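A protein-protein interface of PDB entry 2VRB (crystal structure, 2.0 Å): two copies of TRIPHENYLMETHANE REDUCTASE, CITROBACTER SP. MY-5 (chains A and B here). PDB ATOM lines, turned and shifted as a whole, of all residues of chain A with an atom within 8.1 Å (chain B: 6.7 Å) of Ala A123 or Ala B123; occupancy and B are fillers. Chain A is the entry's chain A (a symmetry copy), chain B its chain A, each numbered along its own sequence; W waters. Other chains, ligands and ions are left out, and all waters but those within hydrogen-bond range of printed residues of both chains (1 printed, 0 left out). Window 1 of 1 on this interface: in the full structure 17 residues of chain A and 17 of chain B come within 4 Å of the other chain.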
ATOM      1  N   ASN A  80       2.096   2.444  19.582  1.00  0.00           N
ATOM      2  CA  ASN A  80       2.813   3.611  20.124  1.00  0.00           C
ATOM      3  C   ASN A  80       4.343   3.527  19.990  1.00  0.00           C
ATOM      4  O   ASN A  80       4.998   4.535  19.784  1.00  0.00           O
ATOM      5  CB  ASN A  80       2.407   3.836  21.590  1.00  0.00           C
ATOM      6  CG  ASN A  80       0.940   4.325  21.716  1.00  0.00           C
ATOM      7  OD1 ASN A  80       0.483   5.112  20.908  1.00  0.00           O
ATOM      8  ND2 ASN A  80       0.231   3.854  22.737  1.00  0.00           N
ATOM      9  N   LEU A  83       5.073   4.256  16.480  1.00  0.00           N
ATOM     10  CA  LEU A  83       4.887   5.696  16.321  1.00  0.00           C
ATOM     11  C   LEU A  83       6.130   6.508  16.775  1.00  0.00           C
ATOM     12  O   LEU A  83       6.454   7.477  16.168  1.00  0.00           O
ATOM     13  CB  LEU A  83       3.628   6.164  17.072  1.00  0.00           C
ATOM     14  CG  LEU A  83       2.860   7.405  16.621  1.00  0.00           C
ATOM     15  CD1 LEU A  83       2.633   7.383  15.096  1.00  0.00           C
ATOM     16  CD2 LEU A  83       1.546   7.590  17.381  1.00  0.00           C
ATOM     17  N   ILE A  84       6.807   6.088  17.825  1.00  0.00           N
ATOM     18  CA  ILE A  84       8.062   6.762  18.247  1.00  0.00           C
ATOM     19  C   ILE A  84       9.153   6.685  17.181  1.00  0.00           C
ATOM     20  O   ILE A  84       9.854   7.667  16.932  1.00  0.00           O
ATOM     21  CB  ILE A  84       8.539   6.238  19.627  1.00  0.00           C
ATOM     22  CG1 ILE A  84       7.487   6.667  20.686  1.00  0.00           C
ATOM     23  CG2 ILE A  84      10.011   6.708  19.986  1.00  0.00           C
ATOM     24  CD1 ILE A  84       8.012   6.927  22.021  1.00  0.00           C
ATOM     25  N   VAL A  85       9.320   5.517  16.562  1.00  0.00           N
ATOM     26  CA  VAL A  85      10.234   5.395  15.409  1.00  0.00           C
ATOM     27  C   VAL A  85       9.844   6.341  14.267  1.00  0.00           C
ATOM     28  O   VAL A  85      10.684   7.053  13.772  1.00  0.00           O
ATOM     29  CB  VAL A  85      10.384   3.922  14.932  1.00  0.00           C
ATOM     30  CG1 VAL A  85      11.394   3.791  13.780  1.00  0.00           C
ATOM     31  CG2 VAL A  85      10.863   3.064  16.077  1.00  0.00           C
ATOM     32  N   HIS A  87       7.930   9.093  14.224  1.00  0.00           N
ATOM     33  CA  HIS A  87       8.122  10.476  14.646  1.00  0.00           C
ATOM     34  C   HIS A  87       9.594  10.805  14.687  1.00  0.00           C
ATOM     35  O   HIS A  87       9.987  11.849  14.214  1.00  0.00           O
ATOM     36  CB  HIS A  87       7.464  10.694  16.027  1.00  0.00           C
ATOM     37  CG  HIS A  87       5.959  10.785  15.959  1.00  0.00           C
ATOM     38  ND1 HIS A  87       5.203  11.365  16.951  1.00  0.00           N
ATOM     39  CD2 HIS A  87       5.088  10.406  14.996  1.00  0.00           C
ATOM     40  CE1 HIS A  87       3.925  11.336  16.608  1.00  0.00           C
ATOM     41  NE2 HIS A  87       3.828  10.760  15.429  1.00  0.00           N
ATOM     42  N   ALA A  88      10.423   9.917  15.213  1.00  0.00           N
ATOM     43  CA  ALA A  88      11.896  10.174  15.188  1.00  0.00           C
ATOM     44  C   ALA A  88      12.489  10.383  13.779  1.00  0.00           C
ATOM     45  O   ALA A  88      13.428  11.204  13.573  1.00  0.00           O
ATOM     46  CB  ALA A  88      12.639   9.053  15.912  1.00  0.00           C
ATOM     47  N   VAL A  91      11.399  13.802  12.612  1.00  0.00           N
ATOM     48  CA  VAL A  91      12.191  14.880  13.211  1.00  0.00           C
ATOM     49  C   VAL A  91      13.580  14.893  12.584  1.00  0.00           C
ATOM     50  O   VAL A  91      14.164  15.972  12.388  1.00  0.00           O
ATOM     51  CB  VAL A  91      12.344  14.739  14.742  1.00  0.00           C
ATOM     52  CG1 VAL A  91      13.234  15.822  15.292  1.00  0.00           C
ATOM     53  CG2 VAL A  91      10.987  14.785  15.427  1.00  0.00           C
ATOM     54  N   TYR A 104       4.312  21.035  16.164  1.00  0.00           N
ATOM     55  CA  TYR A 104       3.956  19.645  16.313  1.00  0.00           C
ATOM     56  C   TYR A 104       2.670  19.562  17.120  1.00  0.00           C
ATOM     57  O   TYR A 104       2.546  20.213  18.150  1.00  0.00           O
ATOM     58  CB  TYR A 104       5.098  18.911  17.039  1.00  0.00           C
ATOM     59  CG  TYR A 104       4.721  17.516  17.487  1.00  0.00           C
ATOM     60  CD1 TYR A 104       4.363  16.536  16.556  1.00  0.00           C
ATOM     61  CD2 TYR A 104       4.687  17.185  18.833  1.00  0.00           C
ATOM     62  CE1 TYR A 104       4.050  15.251  16.941  1.00  0.00           C
ATOM     63  CE2 TYR A 104       4.316  15.898  19.230  1.00  0.00           C
ATOM     64  CZ  TYR A 104       4.015  14.940  18.273  1.00  0.00           C
ATOM     65  OH  TYR A 104       3.609  13.653  18.673  1.00  0.00           O
ATOM     66  N   ALA A 110       0.314  16.594  28.892  1.00  0.00           N
ATOM     67  CA  ALA A 110       0.841  15.260  28.708  1.00  0.00           C
ATOM     68  C   ALA A 110       1.577  14.692  29.936  1.00  0.00           C
ATOM     69  O   ALA A 110       1.465  13.480  30.239  1.00  0.00           O
ATOM     70  CB  ALA A 110       1.742  15.236  27.492  1.00  0.00           C
ATOM     71  N   LEU A 117      -0.339   7.018  24.960  1.00  0.00           N
ATOM     72  CA  LEU A 117      -0.043   7.880  23.851  1.00  0.00           C
ATOM     73  C   LEU A 117       0.590   9.209  24.316  1.00  0.00           C
ATOM     74  O   LEU A 117       1.272   9.869  23.524  1.00  0.00           O
ATOM     75  CB  LEU A 117      -1.304   8.129  22.999  1.00  0.00           C
ATOM     76  CG  LEU A 117      -1.198   9.026  21.775  1.00  0.00           C
ATOM     77  CD1 LEU A 117      -0.110   8.591  20.741  1.00  0.00           C
ATOM     78  CD2 LEU A 117      -2.579   9.156  21.108  1.00  0.00           C
ATOM     79  N   ALA A 118       0.377   9.618  25.575  1.00  0.00           N
ATOM     80  CA  ALA A 118       0.971  10.876  26.016  1.00  0.00           C
ATOM     81  C   ALA A 118       2.512  10.773  26.056  1.00  0.00           C
ATOM     82  O   ALA A 118       3.188  11.753  25.845  1.00  0.00           O
ATOM     83  CB  ALA A 118       0.469  11.242  27.386  1.00  0.00           C
ATOM     84  N   HIS A 119       3.033   9.574  26.296  1.00  0.00           N
ATOM     85  CA  HIS A 119       4.506   9.343  26.342  1.00  0.00           C
ATOM     86  C   HIS A 119       5.091   9.472  24.946  1.00  0.00           C
ATOM     87  O   HIS A 119       6.189   9.885  24.805  1.00  0.00           O
ATOM     88  CB  HIS A 119       4.789   7.934  26.857  1.00  0.00           C
ATOM     89  CG  HIS A 119       4.424   7.753  28.288  1.00  0.00           C
ATOM     90  ND1 HIS A 119       4.018   6.538  28.815  1.00  0.00           N
ATOM     91  CD2 HIS A 119       4.379   8.644  29.301  1.00  0.00           C
ATOM     92  CE1 HIS A 119       3.806   6.688  30.109  1.00  0.00           C
ATOM     93  NE2 HIS A 119       4.016   7.950  30.429  1.00  0.00           N
ATOM     94  N   VAL A 120       4.338   9.104  23.915  1.00  0.00           N
ATOM     95  CA  VAL A 120       4.795   9.296  22.528  1.00  0.00           C
ATOM     96  C   VAL A 120       4.951  10.798  22.222  1.00  0.00           C
ATOM     97  O   VAL A 120       5.913  11.235  21.551  1.00  0.00           O
ATOM     98  CB  VAL A 120       3.783   8.668  21.513  1.00  0.00           C
ATOM     99  CG1 VAL A 120       4.173   8.966  20.070  1.00  0.00           C
ATOM    100  CG2 VAL A 120       3.732   7.161  21.681  1.00  0.00           C
ATOM    101  N   HIS A 121       3.957  11.583  22.634  1.00  0.00           N
ATOM    102  CA  HIS A 121       3.984  13.025  22.328  1.00  0.00           C
ATOM    103  C   HIS A 121       5.118  13.691  23.081  1.00  0.00           C
ATOM    104  O   HIS A 121       5.838  14.529  22.537  1.00  0.00           O
ATOM    105  CB  HIS A 121       2.662  13.701  22.685  1.00  0.00           C
ATOM    106  CG  HIS A 121       1.539  13.287  21.795  1.00  0.00           C
ATOM    107  ND1 HIS A 121       1.639  13.329  20.423  1.00  0.00           N
ATOM    108  CD2 HIS A 121       0.346  12.706  22.075  1.00  0.00           C
ATOM    109  CE1 HIS A 121       0.492  12.901  19.890  1.00  0.00           C
ATOM    110  NE2 HIS A 121      -0.309  12.516  20.872  1.00  0.00           N
ATOM    111  N   LEU A 122       5.277  13.340  24.337  1.00  0.00           N
ATOM    112  CA  LEU A 122       6.523  13.834  25.078  1.00  0.00           C
ATOM    113  C   LEU A 122       7.832  13.365  24.480  1.00  0.00           C
ATOM    114  O   LEU A 122       8.823  14.148  24.411  1.00  0.00           O
ATOM    115  CB  LEU A 122       6.449  13.411  26.524  1.00  0.00           C
ATOM    116  CG  LEU A 122       5.367  14.177  27.299  1.00  0.00           C
ATOM    117  CD1 LEU A 122       4.936  13.383  28.522  1.00  0.00           C
ATOM    118  CD2 LEU A 122       5.942  15.534  27.701  1.00  0.00           C
ATOM    119  N   ALA A 123       7.919  12.090  24.068  1.00  0.00           N
ATOM    120  CA  ALA A 123       9.176  11.649  23.414  1.00  0.00           C
ATOM    121  C   ALA A 123       9.468  12.497  22.190  1.00  0.00           C
ATOM    122  O   ALA A 123      10.616  12.844  21.901  1.00  0.00           O
ATOM    123  CB  ALA A 123       9.106  10.158  23.014  1.00  0.00           C
ATOM    124  N   THR A 124       8.416  12.784  21.440  1.00  0.00           N
ATOM    125  CA  THR A 124       8.522  13.560  20.179  1.00  0.00           C
ATOM    126  C   THR A 124       8.911  15.032  20.437  1.00  0.00           C
ATOM    127  O   THR A 124       9.718  15.606  19.710  1.00  0.00           O
ATOM    128  CB  THR A 124       7.210  13.474  19.378  1.00  0.00           C
ATOM    129  OG1 THR A 124       6.889  12.077  19.140  1.00  0.00           O
ATOM    130  CG2 THR A 124       7.344  14.210  18.041  1.00  0.00           C
ATOM    131  N   GLU A 125       8.304  15.653  21.442  1.00  0.00           N
ATOM    132  CA  GLU A 125       8.647  17.013  21.823  1.00  0.00           C
ATOM    133  C   GLU A 125      10.131  17.073  22.201  1.00  0.00           C
ATOM    134  O   GLU A 125      10.855  17.983  21.782  1.00  0.00           O
ATOM    135  CB  GLU A 125       7.813  17.448  23.028  1.00  0.00           C
ATOM    136  CG  GLU A 125       6.359  17.723  22.666  1.00  0.00           C
ATOM    137  CD  GLU A 125       5.637  18.444  23.788  1.00  0.00           C
ATOM    138  OE1 GLU A 125       6.252  18.810  24.827  1.00  0.00           O
ATOM    139  OE2 GLU A 125       4.439  18.685  23.600  1.00  0.00           O
ATOM    140  N   TYR A 126      10.600  16.109  22.987  1.00  0.00           N
ATOM    141  CA  TYR A 126      12.054  16.081  23.308  1.00  0.00           C
ATOM    142  C   TYR A 126      12.930  15.849  22.091  1.00  0.00           C
ATOM    143  O   TYR A 126      14.035  16.432  21.973  1.00  0.00           O
ATOM    144  CB  TYR A 126      12.369  15.076  24.428  1.00  0.00           C
ATOM    145  CG  TYR A 126      11.994  15.600  25.760  1.00  0.00           C
ATOM    146  CD1 TYR A 126      12.738  16.636  26.361  1.00  0.00           C
ATOM    147  CD2 TYR A 126      10.910  15.085  26.427  1.00  0.00           C
ATOM    148  CE1 TYR A 126      12.355  17.170  27.596  1.00  0.00           C
ATOM    149  CE2 TYR A 126      10.526  15.605  27.682  1.00  0.00           C
ATOM    150  CZ  TYR A 126      11.233  16.647  28.225  1.00  0.00           C
ATOM    151  OH  TYR A 126      10.851  17.136  29.460  1.00  0.00           O
ATOM    152  N   ALA A 127      12.482  14.979  21.191  1.00  0.00           N
ATOM    153  CA  ALA A 127      13.170  14.781  19.895  1.00  0.00           C
ATOM    154  C   ALA A 127      13.292  16.068  19.110  1.00  0.00           C
ATOM    155  O   ALA A 127      14.401  16.405  18.654  1.00  0.00           O
ATOM    156  CB  ALA A 127      12.533  13.731  19.062  1.00  0.00           C
ATOM    157  N   ILE A 128      12.207  16.818  19.012  1.00  0.00           N
ATOM    158  CA  ILE A 128      12.225  18.166  18.392  1.00  0.00           C
ATOM    159  C   ILE A 128      13.152  19.177  19.125  1.00  0.00           C
ATOM    160  O   ILE A 128      13.898  19.966  18.479  1.00  0.00           O
ATOM    161  CB  ILE A 128      10.780  18.705  18.251  1.00  0.00           C
ATOM    162  CG1 ILE A 128      10.034  17.810  17.255  1.00  0.00           C
ATOM    163  CG2 ILE A 128      10.792  20.201  17.842  1.00  0.00           C
ATOM    164  CD1 ILE A 128       8.438  17.973  17.205  1.00  0.00           C
ATOM    165  N   ARG A 129      13.176  19.122  20.457  1.00  0.00           N
ATOM    166  CA  ARG A 129      14.085  20.019  21.206  1.00  0.00           C
ATOM    167  C   ARG A 129      15.527  19.741  20.894  1.00  0.00           C
ATOM    168  O   ARG A 129      16.365  20.668  20.928  1.00  0.00           O
ATOM    169  CB  ARG A 129      13.864  19.955  22.720  1.00  0.00           C
ATOM    170  CG  ARG A 129      12.517  20.568  23.200  1.00  0.00           C
ATOM    171  CD  ARG A 129      12.316  20.408  24.717  1.00  0.00           C
ATOM    172  NE  ARG A 129      10.964  20.816  25.164  1.00  0.00           N
ATOM    173  CZ  ARG A 129      10.657  22.104  25.361  1.00  0.00           C
ATOM    174  NH1 ARG A 129      11.594  23.044  25.132  1.00  0.00           N
ATOM    175  NH2 ARG A 129       9.458  22.464  25.791  1.00  0.00           N
ATOM    176  N   THR A 130      15.842  18.501  20.538  1.00  0.00           N
ATOM    177  CA  THR A 130      17.230  18.157  20.211  1.00  0.00           C
ATOM    178  C   THR A 130      17.679  18.774  18.909  1.00  0.00           C
ATOM    179  O   THR A 130      18.853  18.970  18.719  1.00  0.00           O
ATOM    180  CB  THR A 130      17.462  16.627  20.103  1.00  0.00           C
ATOM    181  OG1 THR A 130      16.822  16.160  18.890  1.00  0.00           O
ATOM    182  CG2 THR A 130      16.888  15.922  21.300  1.00  0.00           C
ATOM    183  N   ILE B  84      18.550   9.822  18.737  1.00  0.00           N
ATOM    184  CA  ILE B  84      17.112   9.556  19.000  1.00  0.00           C
ATOM    185  C   ILE B  84      16.546   8.461  18.096  1.00  0.00           C
ATOM    186  O   ILE B  84      15.790   7.603  18.554  1.00  0.00           O
ATOM    187  CB  ILE B  84      16.283  10.865  18.940  1.00  0.00           C
ATOM    188  CG1 ILE B  84      16.738  11.768  20.119  1.00  0.00           C
ATOM    189  CG2 ILE B  84      14.719  10.600  18.926  1.00  0.00           C
ATOM    190  CD1 ILE B  84      15.707  12.635  20.678  1.00  0.00           C
ATOM    191  N   ALA B 118      20.649  15.949  27.217  1.00  0.00           N
ATOM    192  CA  ALA B 118      19.669  15.551  28.224  1.00  0.00           C
ATOM    193  C   ALA B 118      18.290  15.293  27.576  1.00  0.00           C
ATOM    194  O   ALA B 118      17.542  14.473  28.056  1.00  0.00           O
ATOM    195  CB  ALA B 118      19.526  16.623  29.270  1.00  0.00           C
ATOM    196  N   HIS B 119      17.999  15.981  26.477  1.00  0.00           N
ATOM    197  CA  HIS B 119      16.706  15.807  25.752  1.00  0.00           C
ATOM    198  C   HIS B 119      16.674  14.447  25.077  1.00  0.00           C
ATOM    199  O   HIS B 119      15.647  13.876  24.954  1.00  0.00           O
ATOM    200  CB  HIS B 119      16.573  16.883  24.677  1.00  0.00           C
ATOM    201  CG  HIS B 119      16.406  18.250  25.240  1.00  0.00           C
ATOM    202  ND1 HIS B 119      16.845  19.392  24.589  1.00  0.00           N
ATOM    203  CD2 HIS B 119      15.869  18.657  26.409  1.00  0.00           C
ATOM    204  CE1 HIS B 119      16.518  20.444  25.316  1.00  0.00           C
ATOM    205  NE2 HIS B 119      15.927  20.030  26.421  1.00  0.00           N
ATOM    206  N   VAL B 120      17.820  13.939  24.635  1.00  0.00           N
ATOM    207  CA  VAL B 120      17.885  12.582  24.066  1.00  0.00           C
ATOM    208  C   VAL B 120      17.525  11.536  25.138  1.00  0.00           C
ATOM    209  O   VAL B 120      16.813  10.542  24.872  1.00  0.00           O
ATOM    210  CB  VAL B 120      19.316  12.276  23.511  1.00  0.00           C
ATOM    211  CG1 VAL B 120      19.439  10.834  23.031  1.00  0.00           C
ATOM    212  CG2 VAL B 120      19.634  13.187  22.339  1.00  0.00           C
ATOM    213  N   HIS B 121      18.090  11.707  26.332  1.00  0.00           N
ATOM    214  CA  HIS B 121      17.859  10.719  27.402  1.00  0.00           C
ATOM    215  C   HIS B 121      16.408  10.760  27.837  1.00  0.00           C
ATOM    216  O   HIS B 121      15.777   9.724  28.047  1.00  0.00           O
ATOM    217  CB  HIS B 121      18.766  10.971  28.605  1.00  0.00           C
ATOM    218  CG  HIS B 121      20.201  10.686  28.321  1.00  0.00           C
ATOM    219  ND1 HIS B 121      20.616   9.498  27.766  1.00  0.00           N
ATOM    220  CD2 HIS B 121      21.300  11.479  28.396  1.00  0.00           C
ATOM    221  CE1 HIS B 121      21.943   9.524  27.622  1.00  0.00           C
ATOM    222  NE2 HIS B 121      22.382  10.716  27.997  1.00  0.00           N
ATOM    223  N   LEU B 122      15.873  11.950  27.991  1.00  0.00           N
ATOM    224  CA  LEU B 122      14.364  12.043  28.235  1.00  0.00           C
ATOM    225  C   LEU B 122      13.514  11.488  27.113  1.00  0.00           C
ATOM    226  O   LEU B 122      12.474  10.815  27.368  1.00  0.00           O
ATOM    227  CB  LEU B 122      13.984  13.479  28.494  1.00  0.00           C
ATOM    228  CG  LEU B 122      14.498  13.981  29.852  1.00  0.00           C
ATOM    229  CD1 LEU B 122      14.603  15.499  29.843  1.00  0.00           C
ATOM    230  CD2 LEU B 122      13.527  13.505  30.931  1.00  0.00           C
ATOM    231  N   ALA B 123      13.875  11.766  25.850  1.00  0.00           N
ATOM    232  CA  ALA B 123      13.086  11.162  24.747  1.00  0.00           C
ATOM    233  C   ALA B 123      13.092   9.648  24.851  1.00  0.00           C
ATOM    234  O   ALA B 123      12.090   8.977  24.595  1.00  0.00           O
ATOM    235  CB  ALA B 123      13.630  11.594  23.367  1.00  0.00           C
ATOM    236  N   THR B 124      14.257   9.112  25.182  1.00  0.00           N
ATOM    237  CA  THR B 124      14.460   7.645  25.282  1.00  0.00           C
ATOM    238  C   THR B 124      13.685   7.033  26.470  1.00  0.00           C
ATOM    239  O   THR B 124      13.103   5.957  26.354  1.00  0.00           O
ATOM    240  CB  THR B 124      15.960   7.312  25.379  1.00  0.00           C
ATOM    241  OG1 THR B 124      16.649   7.888  24.237  1.00  0.00           O
ATOM    242  CG2 THR B 124      16.177   5.795  25.403  1.00  0.00           C
ATOM    243  N   GLU B 125      13.717   7.694  27.621  1.00  0.00           N
ATOM    244  CA  GLU B 125      12.963   7.252  28.781  1.00  0.00           C
ATOM    245  C   GLU B 125      11.472   7.207  28.428  1.00  0.00           C
ATOM    246  O   GLU B 125      10.775   6.237  28.749  1.00  0.00           O
ATOM    247  CB  GLU B 125      13.165   8.225  29.943  1.00  0.00           C
ATOM    248  CG  GLU B 125      14.548   8.108  30.571  1.00  0.00           C
ATOM    249  CD  GLU B 125      14.618   8.842  31.896  1.00  0.00           C
ATOM    250  OE1 GLU B 125      13.594   9.389  32.390  1.00  0.00           O
ATOM    251  OE2 GLU B 125      15.713   8.831  32.470  1.00  0.00           O
ATOM    252  N   TYR B 126      10.971   8.243  27.765  1.00  0.00           N
ATOM    253  CA  TYR B 126       9.548   8.202  27.327  1.00  0.00           C
ATOM    254  C   TYR B 126       9.267   7.107  26.314  1.00  0.00           C
ATOM    255  O   TYR B 126       8.187   6.470  26.340  1.00  0.00           O
ATOM    256  CB  TYR B 126       9.069   9.572  26.822  1.00  0.00           C
ATOM    257  CG  TYR B 126       8.791  10.505  27.937  1.00  0.00           C
ATOM    258  CD1 TYR B 126       7.666  10.319  28.766  1.00  0.00           C
ATOM    259  CD2 TYR B 126       9.632  11.562  28.182  1.00  0.00           C
ATOM    260  CE1 TYR B 126       7.429  11.167  29.854  1.00  0.00           C
ATOM    261  CE2 TYR B 126       9.391  12.433  29.266  1.00  0.00           C
ATOM    262  CZ  TYR B 126       8.320  12.205  30.091  1.00  0.00           C
ATOM    263  OH  TYR B 126       8.093  13.075  31.140  1.00  0.00           O
ATOM    264  N   ALA B 127      10.201   6.894  25.393  1.00  0.00           N
ATOM    265  CA  ALA B 127      10.111   5.758  24.447  1.00  0.00           C
ATOM    266  C   ALA B 127      10.008   4.428  25.159  1.00  0.00           C
ATOM    267  O   ALA B 127       9.106   3.630  24.841  1.00  0.00           O
ATOM    268  CB  ALA B 127      11.230   5.733  23.472  1.00  0.00           C
ATOM    269  N   ILE B 128      10.855   4.210  26.152  1.00  0.00           N
ATOM    270  CA  ILE B 128      10.770   3.010  27.021  1.00  0.00           C
ATOM    271  C   ILE B 128       9.436   2.907  27.814  1.00  0.00           C
ATOM    272  O   ILE B 128       8.831   1.804  27.932  1.00  0.00           O
ATOM    273  CB  ILE B 128      12.004   2.943  27.955  1.00  0.00           C
ATOM    274  CG1 ILE B 128      13.247   2.728  27.085  1.00  0.00           C
ATOM    275  CG2 ILE B 128      11.813   1.846  29.035  1.00  0.00           C
ATOM    276  CD1 ILE B 128      14.667   2.960  27.799  1.00  0.00           C
ATOM    277  N   THR B 130       6.636   3.827  26.811  1.00  0.00           N
ATOM    278  CA  THR B 130       5.586   3.418  25.873  1.00  0.00           C
ATOM    279  C   THR B 130       5.533   1.920  25.695  1.00  0.00           C
ATOM    280  O   THR B 130       4.502   1.402  25.342  1.00  0.00           O
ATOM    281  CB  THR B 130       5.759   4.046  24.465  1.00  0.00           C
ATOM    282  OG1 THR B 130       6.892   3.411  23.826  1.00  0.00           O
ATOM    283  CG2 THR B 130       5.984   5.529  24.575  1.00  0.00           C
HETATM  284  O   HOH W   1      18.302  20.535  22.675  1.00  0.00           O
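The side-chain hydroxyl of Thr A130 lies within hydrogen-bond range of the backbone carbonyl oxygen of Ala A127 (2.4 Å). The backbone carbonyl oxygen (O) of Val B120 lies within hydrogen-bond range of the side-chain hydroxyl (OG1) of Thr B124 (2.7 Å). The backbone carbonyl oxygen (O) of Val A120 is in hydrogen-bond range of the side-chain hydroxyl (OG1) of Thr A124, at 2.7 Å. O of Ala B127 sits at hydrogen-bond distance from OG1 of Thr B130 (2.4 Å).
Printed residues of chain B within 4 Å of Ala A88: Ile B84 (3.98 Å). Val A91 touches none of the printed residues of chain B. Ala A110 touches none of the printed residues of chain B. Of chain B, only Ala B123 (3.6 Å) and Tyr B126 (3.9 Å) come within 4 Å of Ala A123. Of the printed residues of chain B, Tyr A126 touches His B119, Leu B122, Ala B123 and Tyr B126. Of the printed residues of chain B, Thr A130 touches Ile B84, His B119 and Val B120. Printed residues of chain A within 4 Å of His B119: Tyr A126, Arg A129 and Thr A130. Of the printed residues of chain A, Leu B122 touches Tyr A126 (3.6 Å). Of chain A, only Ala A123 (3.6 Å) and Tyr A126 (3.9 Å) come within 4 Å of Ala B123. The nearest residue of chain B that does not touch Ala A123 is Ala B127 (4.2 Å). The nearest residue of chain A that does not touch Ala B123 is Ala A127 (4.2 Å).
Among the printed residues, pairs that only touch across the chains: Ala A127 with Ile B84 (3.4 Å), Ile A84 with Ala B127 (3.4 Å), His A119 with Thr B130 (3.5 Å), Thr A130 with His B119 (3.5 Å), His A119 with Tyr B126 (3.5 Å), Tyr A126 with His B119 (3.5 Å), Thr A130 with Ile B84 (3.5 Å), Ile A84 with Thr B130 (3.5 Å), Arg A129 with His B119 (3.6 Å), Ala A123 with Ala B123 (3.6 Å), Tyr A126 with Leu B122 (3.6 Å), Leu A122 with Tyr B126 (3.6 Å), Tyr A126 with Tyr B126 (3.7 Å), Tyr A126 with Ala B123 (3.9 Å), Ala A123 with Tyr B126 (3.9 Å), Ala A88 with Ile B84 (3.98 Å), Thr A130 with Val B120 (3.99 Å) and Val A120 with Thr B130 (3.99 Å).
Ile A84 touches Thr B130, and with the chains exchanged Thr A130 touches Ile B84. Leu A122 touches Tyr B126, and with the chains exchanged Tyr A126 touches Leu B122. Ala A123 touches Tyr B126, and with the chains exchanged Tyr A126 touches Ala B123. Tyr A126 touches its own counterpart, Tyr B126. Of the 18 pairs that touch across the chains among the printed residues, 16 have their exchanged pair printed and touching as well.
Water W1 bridges the backbone carbonyl oxygen of Arg A129 (2.6 Å) and a ring nitrogen (ND1) of His B119 (2.7 Å).
Of the 23 printed residues of chain A, 10 touch a printed residue of chain B. Hydrophobic or aromatic side chains of chain A that line the printed part of chain B: Ile A84, Ala A88, His A119, Leu A122, Ala A123, Tyr A126 and Ala A127. Of the 13 printed residues of chain B, 8 touch a printed residue of chain A. Hydrophobic or aromatic side chains of chain B within 4 Å of the printed part of chain A: Ile B84, His B119, Leu B122, Ala B123, Tyr B126 and Ala B127.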
